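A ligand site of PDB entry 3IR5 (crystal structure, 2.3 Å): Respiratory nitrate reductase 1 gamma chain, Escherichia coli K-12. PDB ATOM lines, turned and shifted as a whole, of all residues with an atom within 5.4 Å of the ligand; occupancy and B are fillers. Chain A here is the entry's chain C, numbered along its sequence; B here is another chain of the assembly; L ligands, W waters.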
ATOM      1  N   ALA A  37      23.936  26.200   0.454  1.00  0.00           N
ATOM      2  CA  ALA A  37      23.227  26.475  -0.795  1.00  0.00           C
ATOM      3  C   ALA A  37      21.876  27.120  -0.492  1.00  0.00           C
ATOM      4  O   ALA A  37      21.307  27.817  -1.333  1.00  0.00           O
ATOM      5  CB  ALA A  37      23.022  25.184  -1.575  1.00  0.00           C
ATOM      6  N   ALA A  38      21.377  26.884   0.712  1.00  0.00           N
ATOM      7  CA  ALA A  38      20.102  27.434   1.136  1.00  0.00           C
ATOM      8  C   ALA A  38      18.961  26.926   0.275  1.00  0.00           C
ATOM      9  O   ALA A  38      18.178  27.714  -0.275  1.00  0.00           O
ATOM     10  CB  ALA A  38      20.147  28.964   1.102  1.00  0.00           C
ATOM     11  N   SER A  39      18.855  25.608   0.157  1.00  0.00           N
ATOM     12  CA  SER A  39      17.794  25.002  -0.646  1.00  0.00           C
ATOM     13  C   SER A  39      16.425  25.363  -0.082  1.00  0.00           C
ATOM     14  O   SER A  39      16.261  25.508   1.123  1.00  0.00           O
ATOM     15  CB  SER A  39      17.947  23.479  -0.653  1.00  0.00           C
ATOM     16  OG  SER A  39      16.854  22.897  -1.339  1.00  0.00           O
ATOM     17  N   SER A  40      15.450  25.500  -0.974  1.00  0.00           N
ATOM     18  CA  SER A  40      14.090  25.850  -0.579  1.00  0.00           C
ATOM     19  C   SER A  40      13.160  24.853  -1.248  1.00  0.00           C
ATOM     20  O   SER A  40      11.944  24.925  -1.134  1.00  0.00           O
ATOM     21  CB  SER A  40      13.748  27.268  -1.068  1.00  0.00           C
ATOM     22  OG  SER A  40      13.834  27.358  -2.479  1.00  0.00           O
ATOM     23  N   GLN A  41      13.779  23.904  -1.948  1.00  0.00           N
ATOM     24  CA  GLN A  41      13.058  22.889  -2.682  1.00  0.00           C
ATOM     25  C   GLN A  41      11.976  22.181  -1.851  1.00  0.00           C
ATOM     26  O   GLN A  41      10.841  22.052  -2.286  1.00  0.00           O
ATOM     27  CB  GLN A  41      14.034  21.851  -3.229  1.00  0.00           C
ATOM     28  CG  GLN A  41      13.528  21.138  -4.473  1.00  0.00           C
ATOM     29  CD  GLN A  41      14.308  19.879  -4.792  1.00  0.00           C
ATOM     30  OE1 GLN A  41      15.520  19.790  -4.561  1.00  0.00           O
ATOM     31  NE2 GLN A  41      13.620  18.895  -5.337  1.00  0.00           N
ATOM     32  N   MET A  48      10.373  23.493  -9.470  1.00  0.00           N
ATOM     33  CA  MET A  48      11.801  23.560  -9.157  1.00  0.00           C
ATOM     34  C   MET A  48      12.685  22.687 -10.029  1.00  0.00           C
ATOM     35  O   MET A  48      13.835  23.040 -10.317  1.00  0.00           O
ATOM     36  CB  MET A  48      12.037  23.205  -7.676  1.00  0.00           C
ATOM     37  CG  MET A  48      11.941  24.387  -6.764  1.00  0.00           C
ATOM     38  SD  MET A  48      12.973  25.729  -7.392  1.00  0.00           S
ATOM     39  CE  MET A  48      14.524  25.445  -6.485  1.00  0.00           C
ATOM     40  N   SER A  52      15.176  25.205 -11.754  1.00  0.00           N
ATOM     41  CA  SER A  52      16.569  25.179 -11.314  1.00  0.00           C
ATOM     42  C   SER A  52      17.522  24.576 -12.344  1.00  0.00           C
ATOM     43  O   SER A  52      18.621  25.087 -12.548  1.00  0.00           O
ATOM     44  CB  SER A  52      16.720  24.423  -9.986  1.00  0.00           C
ATOM     45  OG  SER A  52      18.023  24.591  -9.453  1.00  0.00           O
ATOM     46  N   PHE A  55      18.020  27.075 -15.226  1.00  0.00           N
ATOM     47  CA  PHE A  55      18.891  28.124 -14.752  1.00  0.00           C
ATOM     48  C   PHE A  55      20.337  27.690 -14.540  1.00  0.00           C
ATOM     49  O   PHE A  55      21.251  28.370 -15.013  1.00  0.00           O
ATOM     50  CB  PHE A  55      18.335  28.735 -13.460  1.00  0.00           C
ATOM     51  CG  PHE A  55      19.253  29.726 -12.827  1.00  0.00           C
ATOM     52  CD1 PHE A  55      20.131  29.341 -11.824  1.00  0.00           C
ATOM     53  CD2 PHE A  55      19.261  31.047 -13.247  1.00  0.00           C
ATOM     54  CE1 PHE A  55      21.003  30.251 -11.252  1.00  0.00           C
ATOM     55  CE2 PHE A  55      20.131  31.972 -12.691  1.00  0.00           C
ATOM     56  CZ  PHE A  55      21.002  31.575 -11.686  1.00  0.00           C
ATOM     57  N   HIS A  56      20.546  26.582 -13.847  1.00  0.00           N
ATOM     58  CA  HIS A  56      21.922  26.150 -13.587  1.00  0.00           C
ATOM     59  C   HIS A  56      22.671  25.604 -14.791  1.00  0.00           C
ATOM     60  O   HIS A  56      23.847  25.933 -14.983  1.00  0.00           O
ATOM     61  CB  HIS A  56      21.971  25.137 -12.424  1.00  0.00           C
ATOM     62  CG  HIS A  56      21.932  25.765 -11.069  1.00  0.00           C
ATOM     63  ND1 HIS A  56      20.760  25.979 -10.382  1.00  0.00           N
ATOM     64  CD2 HIS A  56      22.918  26.263 -10.281  1.00  0.00           C
ATOM     65  CE1 HIS A  56      21.021  26.588  -9.235  1.00  0.00           C
ATOM     66  NE2 HIS A  56      22.323  26.769  -9.154  1.00  0.00           N
ATOM     67  N   ILE A  59      23.345  28.955 -16.883  1.00  0.00           N
ATOM     68  CA  ILE A  59      24.384  29.829 -16.367  1.00  0.00           C
ATOM     69  C   ILE A  59      25.765  29.189 -16.335  1.00  0.00           C
ATOM     70  O   ILE A  59      26.786  29.891 -16.352  1.00  0.00           O
ATOM     71  CB  ILE A  59      24.044  30.355 -14.953  1.00  0.00           C
ATOM     72  CG1 ILE A  59      24.902  31.596 -14.649  1.00  0.00           C
ATOM     73  CG2 ILE A  59      24.346  29.271 -13.898  1.00  0.00           C
ATOM     74  CD1 ILE A  59      24.169  32.668 -13.874  1.00  0.00           C
ATOM     75  N   LEU A  60      25.806  27.862 -16.256  1.00  0.00           N
ATOM     76  CA  LEU A  60      27.093  27.164 -16.239  1.00  0.00           C
ATOM     77  C   LEU A  60      27.682  27.096 -17.648  1.00  0.00           C
ATOM     78  O   LEU A  60      28.892  26.978 -17.820  1.00  0.00           O
ATOM     79  CB  LEU A  60      26.929  25.761 -15.646  1.00  0.00           C
ATOM     80  CG  LEU A  60      26.924  25.741 -14.115  1.00  0.00           C
ATOM     81  CD1 LEU A  60      26.350  24.423 -13.598  1.00  0.00           C
ATOM     82  CD2 LEU A  60      28.343  25.961 -13.588  1.00  0.00           C
ATOM     83  N   LEU A 108      12.374  30.901 -11.278  1.00  0.00           N
ATOM     84  CA  LEU A 108      12.820  30.840  -9.906  1.00  0.00           C
ATOM     85  C   LEU A 108      12.394  32.095  -9.159  1.00  0.00           C
ATOM     86  O   LEU A 108      12.005  32.031  -7.985  1.00  0.00           O
ATOM     87  CB  LEU A 108      14.342  30.690  -9.854  1.00  0.00           C
ATOM     88  CG  LEU A 108      14.876  29.306 -10.245  1.00  0.00           C
ATOM     89  CD1 LEU A 108      16.388  29.346 -10.427  1.00  0.00           C
ATOM     90  CD2 LEU A 108      14.495  28.315  -9.171  1.00  0.00           C
ATOM     91  N   ARG A 111       8.726  32.294  -8.430  1.00  0.00           N
ATOM     92  CA  ARG A 111       8.503  31.378  -7.328  1.00  0.00           C
ATOM     93  C   ARG A 111       8.864  32.040  -6.001  1.00  0.00           C
ATOM     94  O   ARG A 111       8.057  32.060  -5.074  1.00  0.00           O
ATOM     95  CB  ARG A 111       9.353  30.122  -7.539  1.00  0.00           C
ATOM     96  CG  ARG A 111       9.297  29.090  -6.433  1.00  0.00           C
ATOM     97  CD  ARG A 111       9.952  27.803  -6.900  1.00  0.00           C
ATOM     98  NE  ARG A 111      10.130  26.833  -5.819  1.00  0.00           N
ATOM     99  CZ  ARG A 111      10.992  26.983  -4.820  1.00  0.00           C
ATOM    100  NH1 ARG A 111      11.077  26.049  -3.882  1.00  0.00           N
ATOM    101  NH2 ARG A 111      11.781  28.044  -4.756  1.00  0.00           N
ATOM    102  N   ARG A 112      10.067  32.605  -5.932  1.00  0.00           N
ATOM    103  CA  ARG A 112      10.554  33.252  -4.715  1.00  0.00           C
ATOM    104  C   ARG A 112       9.679  34.408  -4.276  1.00  0.00           C
ATOM    105  O   ARG A 112       9.505  34.646  -3.076  1.00  0.00           O
ATOM    106  CB  ARG A 112      11.987  33.736  -4.924  1.00  0.00           C
ATOM    107  CG  ARG A 112      12.625  34.418  -3.710  1.00  0.00           C
ATOM    108  CD  ARG A 112      14.144  34.413  -3.842  1.00  0.00           C
ATOM    109  NE  ARG A 112      14.645  33.045  -3.879  1.00  0.00           N
ATOM    110  CZ  ARG A 112      14.627  32.217  -2.836  1.00  0.00           C
ATOM    111  NH1 ARG A 112      14.147  32.623  -1.665  1.00  0.00           N
ATOM    112  NH2 ARG A 112      15.060  30.968  -2.962  1.00  0.00           N
ATOM    113  N   ASP A 126      18.650  36.962  -1.021  1.00  0.00           N
ATOM    114  CA  ASP A 126      18.238  35.965  -1.995  1.00  0.00           C
ATOM    115  C   ASP A 126      17.429  36.603  -3.118  1.00  0.00           C
ATOM    116  O   ASP A 126      17.542  36.202  -4.274  1.00  0.00           O
ATOM    117  CB  ASP A 126      17.431  34.857  -1.332  1.00  0.00           C
ATOM    118  CG  ASP A 126      18.203  34.140  -0.228  1.00  0.00           C
ATOM    119  OD1 ASP A 126      19.400  33.858  -0.427  1.00  0.00           O
ATOM    120  OD2 ASP A 126      17.603  33.858   0.838  1.00  0.00           O
ATOM    121  N   ILE A 129      20.160  39.217  -5.124  1.00  0.00           N
ATOM    122  CA  ILE A 129      21.100  38.465  -5.954  1.00  0.00           C
ATOM    123  C   ILE A 129      20.438  37.803  -7.165  1.00  0.00           C
ATOM    124  O   ILE A 129      20.935  37.914  -8.287  1.00  0.00           O
ATOM    125  CB  ILE A 129      21.862  37.418  -5.090  1.00  0.00           C
ATOM    126  CG1 ILE A 129      23.276  37.219  -5.640  1.00  0.00           C
ATOM    127  CG2 ILE A 129      21.119  36.107  -5.047  1.00  0.00           C
ATOM    128  CD1 ILE A 129      24.159  38.458  -5.506  1.00  0.00           C
ATOM    129  N   LEU A 130      19.314  37.131  -6.953  1.00  0.00           N
ATOM    130  CA  LEU A 130      18.602  36.477  -8.051  1.00  0.00           C
ATOM    131  C   LEU A 130      18.111  37.504  -9.059  1.00  0.00           C
ATOM    132  O   LEU A 130      18.189  37.298 -10.264  1.00  0.00           O
ATOM    133  CB  LEU A 130      17.410  35.675  -7.523  1.00  0.00           C
ATOM    134  CG  LEU A 130      16.571  35.037  -8.625  1.00  0.00           C
ATOM    135  CD1 LEU A 130      17.399  33.990  -9.330  1.00  0.00           C
ATOM    136  CD2 LEU A 130      15.295  34.435  -8.047  1.00  0.00           C
ATOM    137  N   LEU A 133      20.898  38.759 -11.232  1.00  0.00           N
ATOM    138  CA  LEU A 133      21.357  37.740 -12.176  1.00  0.00           C
ATOM    139  C   LEU A 133      20.407  37.697 -13.370  1.00  0.00           C
ATOM    140  O   LEU A 133      20.841  37.629 -14.525  1.00  0.00           O
ATOM    141  CB  LEU A 133      21.401  36.362 -11.504  1.00  0.00           C
ATOM    142  CG  LEU A 133      22.580  36.077 -10.575  1.00  0.00           C
ATOM    143  CD1 LEU A 133      22.268  34.843  -9.751  1.00  0.00           C
ATOM    144  CD2 LEU A 133      23.852  35.885 -11.385  1.00  0.00           C
ATOM    145  N   ARG A 202      24.163  34.122  -1.189  1.00  0.00           N
ATOM    146  CA  ARG A 202      24.109  32.675  -1.231  1.00  0.00           C
ATOM    147  C   ARG A 202      25.080  32.148  -2.292  1.00  0.00           C
ATOM    148  O   ARG A 202      25.376  30.955  -2.335  1.00  0.00           O
ATOM    149  CB  ARG A 202      22.688  32.233  -1.577  1.00  0.00           C
ATOM    150  CG  ARG A 202      22.220  32.656  -2.957  1.00  0.00           C
ATOM    151  CD  ARG A 202      20.756  32.310  -3.153  1.00  0.00           C
ATOM    152  NE  ARG A 202      20.505  30.893  -2.938  1.00  0.00           N
ATOM    153  CZ  ARG A 202      19.295  30.387  -2.715  1.00  0.00           C
ATOM    154  NH1 ARG A 202      18.242  31.182  -2.671  1.00  0.00           N
ATOM    155  NH2 ARG A 202      19.144  29.075  -2.528  1.00  0.00           N
ATOM    156  N   LEU A 203      25.587  33.050  -3.130  1.00  0.00           N
ATOM    157  CA  LEU A 203      26.503  32.661  -4.197  1.00  0.00           C
ATOM    158  C   LEU A 203      27.775  31.967  -3.723  1.00  0.00           C
ATOM    159  O   LEU A 203      28.508  31.409  -4.534  1.00  0.00           O
ATOM    160  CB  LEU A 203      26.878  33.882  -5.054  1.00  0.00           C
ATOM    161  CG  LEU A 203      25.697  34.538  -5.771  1.00  0.00           C
ATOM    162  CD1 LEU A 203      26.219  35.610  -6.719  1.00  0.00           C
ATOM    163  CD2 LEU A 203      24.898  33.493  -6.545  1.00  0.00           C
ATOM    164  N   HIS A 205      27.985  29.241  -2.462  1.00  0.00           N
ATOM    165  CA  HIS A 205      27.893  27.794  -2.712  1.00  0.00           C
ATOM    166  C   HIS A 205      28.751  27.379  -3.897  1.00  0.00           C
ATOM    167  O   HIS A 205      29.254  26.262  -3.955  1.00  0.00           O
ATOM    168  CB  HIS A 205      26.432  27.318  -2.918  1.00  0.00           C
ATOM    169  CG  HIS A 205      25.770  27.773  -4.192  1.00  0.00           C
ATOM    170  ND1 HIS A 205      25.546  29.103  -4.473  1.00  0.00           N
ATOM    171  CD2 HIS A 205      25.148  27.072  -5.182  1.00  0.00           C
ATOM    172  CE1 HIS A 205      24.818  29.207  -5.577  1.00  0.00           C
ATOM    173  NE2 HIS A 205      24.563  27.984  -6.025  1.00  0.00           N
ATOM    174  N   ILE A 206      28.946  28.314  -4.831  1.00  0.00           N
ATOM    175  CA  ILE A 206      29.741  28.067  -6.020  1.00  0.00           C
ATOM    176  C   ILE A 206      31.139  27.606  -5.655  1.00  0.00           C
ATOM    177  O   ILE A 206      31.692  26.713  -6.308  1.00  0.00           O
ATOM    178  CB  ILE A 206      29.817  29.332  -6.909  1.00  0.00           C
ATOM    179  CG1 ILE A 206      28.407  29.852  -7.175  1.00  0.00           C
ATOM    180  CG2 ILE A 206      30.507  29.008  -8.231  1.00  0.00           C
ATOM    181  CD1 ILE A 206      28.391  31.157  -7.935  1.00  0.00           C
ATOM    182  N   VAL A 209      31.517  23.605  -5.249  1.00  0.00           N
ATOM    183  CA  VAL A 209      31.159  22.602  -6.243  1.00  0.00           C
ATOM    184  C   VAL A 209      31.928  21.330  -5.847  1.00  0.00           C
ATOM    185  O   VAL A 209      33.147  21.271  -5.912  1.00  0.00           O
ATOM    186  CB  VAL A 209      31.512  23.086  -7.697  1.00  0.00           C
ATOM    187  CG1 VAL A 209      32.927  23.607  -7.748  1.00  0.00           C
ATOM    188  CG2 VAL A 209      31.318  21.960  -8.693  1.00  0.00           C
ATOM    189  N   PRO A 210      31.196  20.293  -5.385  1.00  0.00           N
ATOM    190  CA  PRO A 210      31.686  18.988  -4.924  1.00  0.00           C
ATOM    191  C   PRO A 210      32.426  18.100  -5.917  1.00  0.00           C
ATOM    192  O   PRO A 210      32.033  16.952  -6.142  1.00  0.00           O
ATOM    193  CB  PRO A 210      30.412  18.313  -4.407  1.00  0.00           C
ATOM    194  CG  PRO A 210      29.383  18.803  -5.377  1.00  0.00           C
ATOM    195  CD  PRO A 210      29.723  20.282  -5.499  1.00  0.00           C
ATOM    196  N   ILE B  88      21.961  17.282  -8.587  1.00  0.00           N
ATOM    197  CA  ILE B  88      22.164  18.295  -7.562  1.00  0.00           C
ATOM    198  C   ILE B  88      21.396  19.620  -7.665  1.00  0.00           C
ATOM    199  O   ILE B  88      21.016  20.179  -6.643  1.00  0.00           O
ATOM    200  CB  ILE B  88      23.675  18.573  -7.391  1.00  0.00           C
ATOM    201  CG1 ILE B  88      23.942  19.040  -5.967  1.00  0.00           C
ATOM    202  CG2 ILE B  88      24.140  19.608  -8.413  1.00  0.00           C
ATOM    203  CD1 ILE B  88      25.401  19.022  -5.584  1.00  0.00           C
ATOM    204  N   PHE B  89      21.147  20.131  -8.869  1.00  0.00           N
ATOM    205  CA  PHE B  89      20.430  21.398  -8.978  1.00  0.00           C
ATOM    206  C   PHE B  89      19.003  21.294  -8.472  1.00  0.00           C
ATOM    207  O   PHE B  89      18.395  22.296  -8.114  1.00  0.00           O
ATOM    208  CB  PHE B  89      20.441  21.897 -10.425  1.00  0.00           C
ATOM    209  CG  PHE B  89      21.821  22.008 -10.998  1.00  0.00           C
ATOM    210  CD1 PHE B  89      22.802  22.724 -10.332  1.00  0.00           C
ATOM    211  CD2 PHE B  89      22.145  21.354 -12.172  1.00  0.00           C
ATOM    212  CE1 PHE B  89      24.092  22.779 -10.827  1.00  0.00           C
ATOM    213  CE2 PHE B  89      23.441  21.398 -12.672  1.00  0.00           C
ATOM    214  CZ  PHE B  89      24.410  22.113 -12.000  1.00  0.00           C
ATOM    215  N   ALA B  90      18.477  20.080  -8.439  1.00  0.00           N
ATOM    216  CA  ALA B  90      17.123  19.824  -7.954  1.00  0.00           C
ATOM    217  C   ALA B  90      16.919  18.324  -7.712  1.00  0.00           C
ATOM    218  O   ALA B  90      16.632  17.565  -8.639  1.00  0.00           O
ATOM    219  CB  ALA B  90      16.104  20.354  -8.943  1.00  0.00           C
ATOM    220  N   GLY B 219      24.579  21.843   2.392  1.00  0.00           N
ATOM    221  CA  GLY B 219      23.172  21.904   2.048  1.00  0.00           C
ATOM    222  C   GLY B 219      22.789  21.330   0.694  1.00  0.00           C
ATOM    223  O   GLY B 219      21.768  21.724   0.123  1.00  0.00           O
ATOM    224  N   TRP B 220      23.604  20.402   0.179  1.00  0.00           N
ATOM    225  CA  TRP B 220      23.334  19.770  -1.116  1.00  0.00           C
ATOM    226  C   TRP B 220      22.079  18.896  -1.070  1.00  0.00           C
ATOM    227  O   TRP B 220      21.596  18.422  -2.104  1.00  0.00           O
ATOM    228  CB  TRP B 220      24.517  18.898  -1.554  1.00  0.00           C
ATOM    229  CG  TRP B 220      25.821  19.627  -1.728  1.00  0.00           C
ATOM    230  CD1 TRP B 220      27.047  19.211  -1.315  1.00  0.00           C
ATOM    231  CD2 TRP B 220      26.031  20.886  -2.386  1.00  0.00           C
ATOM    232  NE1 TRP B 220      28.015  20.111  -1.668  1.00  0.00           N
ATOM    233  CE2 TRP B 220      27.412  21.152  -2.329  1.00  0.00           C
ATOM    234  CE3 TRP B 220      25.186  21.807  -3.013  1.00  0.00           C
ATOM    235  CZ2 TRP B 220      27.977  22.310  -2.882  1.00  0.00           C
ATOM    236  CZ3 TRP B 220      25.748  22.957  -3.571  1.00  0.00           C
ATOM    237  CH2 TRP B 220      27.125  23.195  -3.497  1.00  0.00           C
ATOM    238  N   ARG B 221      21.563  18.693   0.135  1.00  0.00           N
ATOM    239  CA  ARG B 221      20.367  17.880   0.387  1.00  0.00           C
ATOM    240  C   ARG B 221      20.161  16.620  -0.462  1.00  0.00           C
ATOM    241  O   ARG B 221      19.060  16.369  -0.966  1.00  0.00           O
ATOM    242  CB  ARG B 221      19.115  18.776   0.314  1.00  0.00           C
ATOM    243  CG  ARG B 221      19.038  19.675  -0.913  1.00  0.00           C
ATOM    244  CD  ARG B 221      18.156  19.086  -2.001  1.00  0.00           C
ATOM    245  NE  ARG B 221      18.007  19.995  -3.122  1.00  0.00           N
ATOM    246  CZ  ARG B 221      18.932  20.210  -4.059  1.00  0.00           C
ATOM    247  NH1 ARG B 221      20.092  19.558  -4.000  1.00  0.00           N
ATOM    248  NH2 ARG B 221      18.704  21.074  -5.040  1.00  0.00           N
HETATM  249  C1  LIG L   1      20.611  27.672  -5.851  1.00  0.00           C
HETATM  250  C2  LIG L   1      23.800  24.121  -6.541  1.00  0.00           C
HETATM  251  C3  LIG L   1      26.320  27.115  -9.389  1.00  0.00           C
HETATM  252  C4  LIG L   1      23.157  30.656  -8.669  1.00  0.00           C
HETATM  253  C5  LIG L   1      21.236  26.440  -5.769  1.00  0.00           C
HETATM  254  C6  LIG L   1      20.797  25.277  -5.014  1.00  0.00           C
HETATM  255  C7  LIG L   1      21.680  24.293  -5.206  1.00  0.00           C
HETATM  256  C8  LIG L   1      22.701  24.825  -6.092  1.00  0.00           C
HETATM  257  C9  LIG L   1      21.690  22.829  -4.645  1.00  0.00           C
HETATM  258  C10 LIG L   1      19.521  25.224  -4.141  1.00  0.00           C
HETATM  259  C11 LIG L   1      18.288  24.693  -4.979  1.00  0.00           C
HETATM  260  C12 LIG L   1      17.045  24.287  -4.178  1.00  0.00           C
HETATM  261  O1  LIG L   1      16.857  23.058  -3.989  1.00  0.00           O
HETATM  262  O2  LIG L   1      16.332  25.249  -3.738  1.00  0.00           O
HETATM  263  C13 LIG L   1      24.766  24.614  -7.387  1.00  0.00           C
HETATM  264  C14 LIG L   1      25.946  23.866  -7.857  1.00  0.00           C
HETATM  265  C15 LIG L   1      26.656  24.709  -8.663  1.00  0.00           C
HETATM  266  C16 LIG L   1      25.929  25.992  -8.689  1.00  0.00           C
HETATM  267  C17 LIG L   1      26.227  22.380  -7.453  1.00  0.00           C
HETATM  268  C18 LIG L   1      28.010  24.440  -9.440  1.00  0.00           C
HETATM  269  C19 LIG L   1      28.279  23.320 -10.187  1.00  0.00           C
HETATM  270  C20 LIG L   1      25.698  28.332  -9.454  1.00  0.00           C
HETATM  271  C21 LIG L   1      26.164  29.504 -10.217  1.00  0.00           C
HETATM  272  C22 LIG L   1      25.281  30.489 -10.011  1.00  0.00           C
HETATM  273  C23 LIG L   1      24.247  29.957  -9.118  1.00  0.00           C
HETATM  274  C24 LIG L   1      27.466  29.519 -11.092  1.00  0.00           C
HETATM  275  C25 LIG L   1      25.246  31.951 -10.558  1.00  0.00           C
HETATM  276  C26 LIG L   1      26.184  32.835 -10.117  1.00  0.00           C
HETATM  277  C27 LIG L   1      22.183  30.166  -7.837  1.00  0.00           C
HETATM  278  C28 LIG L   1      21.018  30.920  -7.382  1.00  0.00           C
HETATM  279  C29 LIG L   1      20.299  30.077  -6.605  1.00  0.00           C
HETATM  280  C30 LIG L   1      21.023  28.790  -6.557  1.00  0.00           C
HETATM  281  C31 LIG L   1      20.700  32.405  -7.751  1.00  0.00           C
HETATM  282  C32 LIG L   1      18.950  30.264  -5.831  1.00  0.00           C
HETATM  283  C33 LIG L   1      17.670  30.282  -6.739  1.00  0.00           C
HETATM  284  C34 LIG L   1      16.393  30.700  -5.996  1.00  0.00           C
HETATM  285  O3  LIG L   1      15.626  29.755  -5.641  1.00  0.00           O
HETATM  286  O4  LIG L   1      16.240  31.959  -5.810  1.00  0.00           O
HETATM  287  N1  LIG L   1      22.408  26.143  -6.423  1.00  0.00           N
HETATM  288  N2  LIG L   1      24.790  25.906  -7.910  1.00  0.00           N
HETATM  289  N3  LIG L   1      24.528  28.636  -8.794  1.00  0.00           N
HETATM  290  N4  LIG L   1      22.147  28.871  -7.322  1.00  0.00           N
HETATM  291 FE1  LIG L   1      23.442  27.374  -7.586  1.00  0.00          FE
HETATM  292  O   HOH W   1      12.918  29.980  -6.050  1.00  0.00           O
HETATM  293  O   HOH W   2      16.156  27.966  -3.598  1.00  0.00           O
HETATM  294  O   HOH W   3      22.500  28.962  -3.687  1.00  0.00           O
HETATM  295  O   HOH W   4      18.049  33.596  -4.903  1.00  0.00           O
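Merely in contact with the ligand: Ala 37 (3.97 Å), Met 48 (3.3 Å), Phe 55 (3.4 Å), Ile 59 (3.6 Å), Leu 108 (3.98 Å), Leu 130 (3.5 Å), Leu 133 (3.5 Å), Leu 203 (3.9 Å), Ile 206 (3.5 Å), Val 209 (3.6 Å), Ile 88 of chain B (3.4 Å), Phe 89 of chain B (3.7 Å) and Trp 220 of chain B (3.7 Å). Hydrophobic or aromatic side chains that line the ligand: Ala 37, Met 48, Phe 55, His 56, Ile 59, Leu 108, Leu 130, Leu 133, Leu 203, His 205, Ile 206, Val 209, Ile 88 of chain B, Phe 89 of chain B and Trp 220 of chain B. The nearest printed residue that does not touch the ligand is Leu 60 (4.1 Å).
A ring nitrogen (NE2) of His 205 binds an iron atom (FE1) of the ligand. NE2 of His 56 binds FE1 of the ligand. An oxygen (O1) of the ligand lies within hydrogen-bond range of the side-chain hydroxyl (OG) of Ser 39 (2.7 Å). NE of Arg 112 is in salt-bridge range of O4 of the ligand, 2.7 Å away. An oxygen (O1) of the ligand is in salt-bridge range of the guanidinium group of Arg 221 of chain B. The backbone NH (N) of Ser 40 sits at hydrogen-bond distance from an oxygen (O2) of the ligand (2.9 Å). The guanidinium group (NH1) of Arg 202 is in salt-bridge range of an oxygen (O4) of the ligand (3.8 Å). The backbone NH of Gln 41 sits at hydrogen-bond distance from an oxygen (O2) of the ligand (3.4 Å).
Water W4 lies within hydrogen-bond range of an oxygen (O4) of the ligand (2.6 Å), the backbone carbonyl oxygen (O) of Asp 126 (2.7 Å) and the guanidinium group (NH1) of Arg 202 (3.3 Å). Water W2 lies within hydrogen-bond range of the side-chain hydroxyl (OG) of Ser 40 (2.6 Å), an oxygen (O2) of the ligand (2.7 Å), the guanidinium group (NH2) of Arg 112 (3.3 Å) and the guanidinium group (NH2) of Arg 202 (3.4 Å). Water W1 lies within hydrogen-bond range of the guanidinium group of Arg 111 (2.6 Å), an oxygen (O3) of the ligand (2.7 Å) and the backbone carbonyl oxygen of Leu 108 (3.0 Å). Water W3 lies within hydrogen-bond range of NE of Arg 202, O of Ala 37 and ND1 of His 205.
O of Arg 202 lies within hydrogen-bond range of ND1 of His 205, at 2.8 Å. A ring nitrogen (ND1) of His 56 sits at hydrogen-bond distance from the backbone carbonyl oxygen (O) of Ser 52. The side-chain hydroxyl of Ser 39 lies within hydrogen-bond range of the backbone NH of Gln 41 (3.3 Å). The guanidinium group (NE) of Arg 221 of chain B is in hydrogen-bond range of the side-chain amide oxygen (OE1) of Gln 41 (2.9 Å). NH2 of Arg 202 lies within hydrogen-bond range of O of Ala 37. OD1 of Asp 126 is in salt-bridge range of NH1 of Arg 202, at 3.7 Å. NE of Arg 111 lies close to SD of Met 48 (3.4 Å). O of Phe 89 of chain B is in hydrogen-bond range of OG of Ser 52 (2.7 Å).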
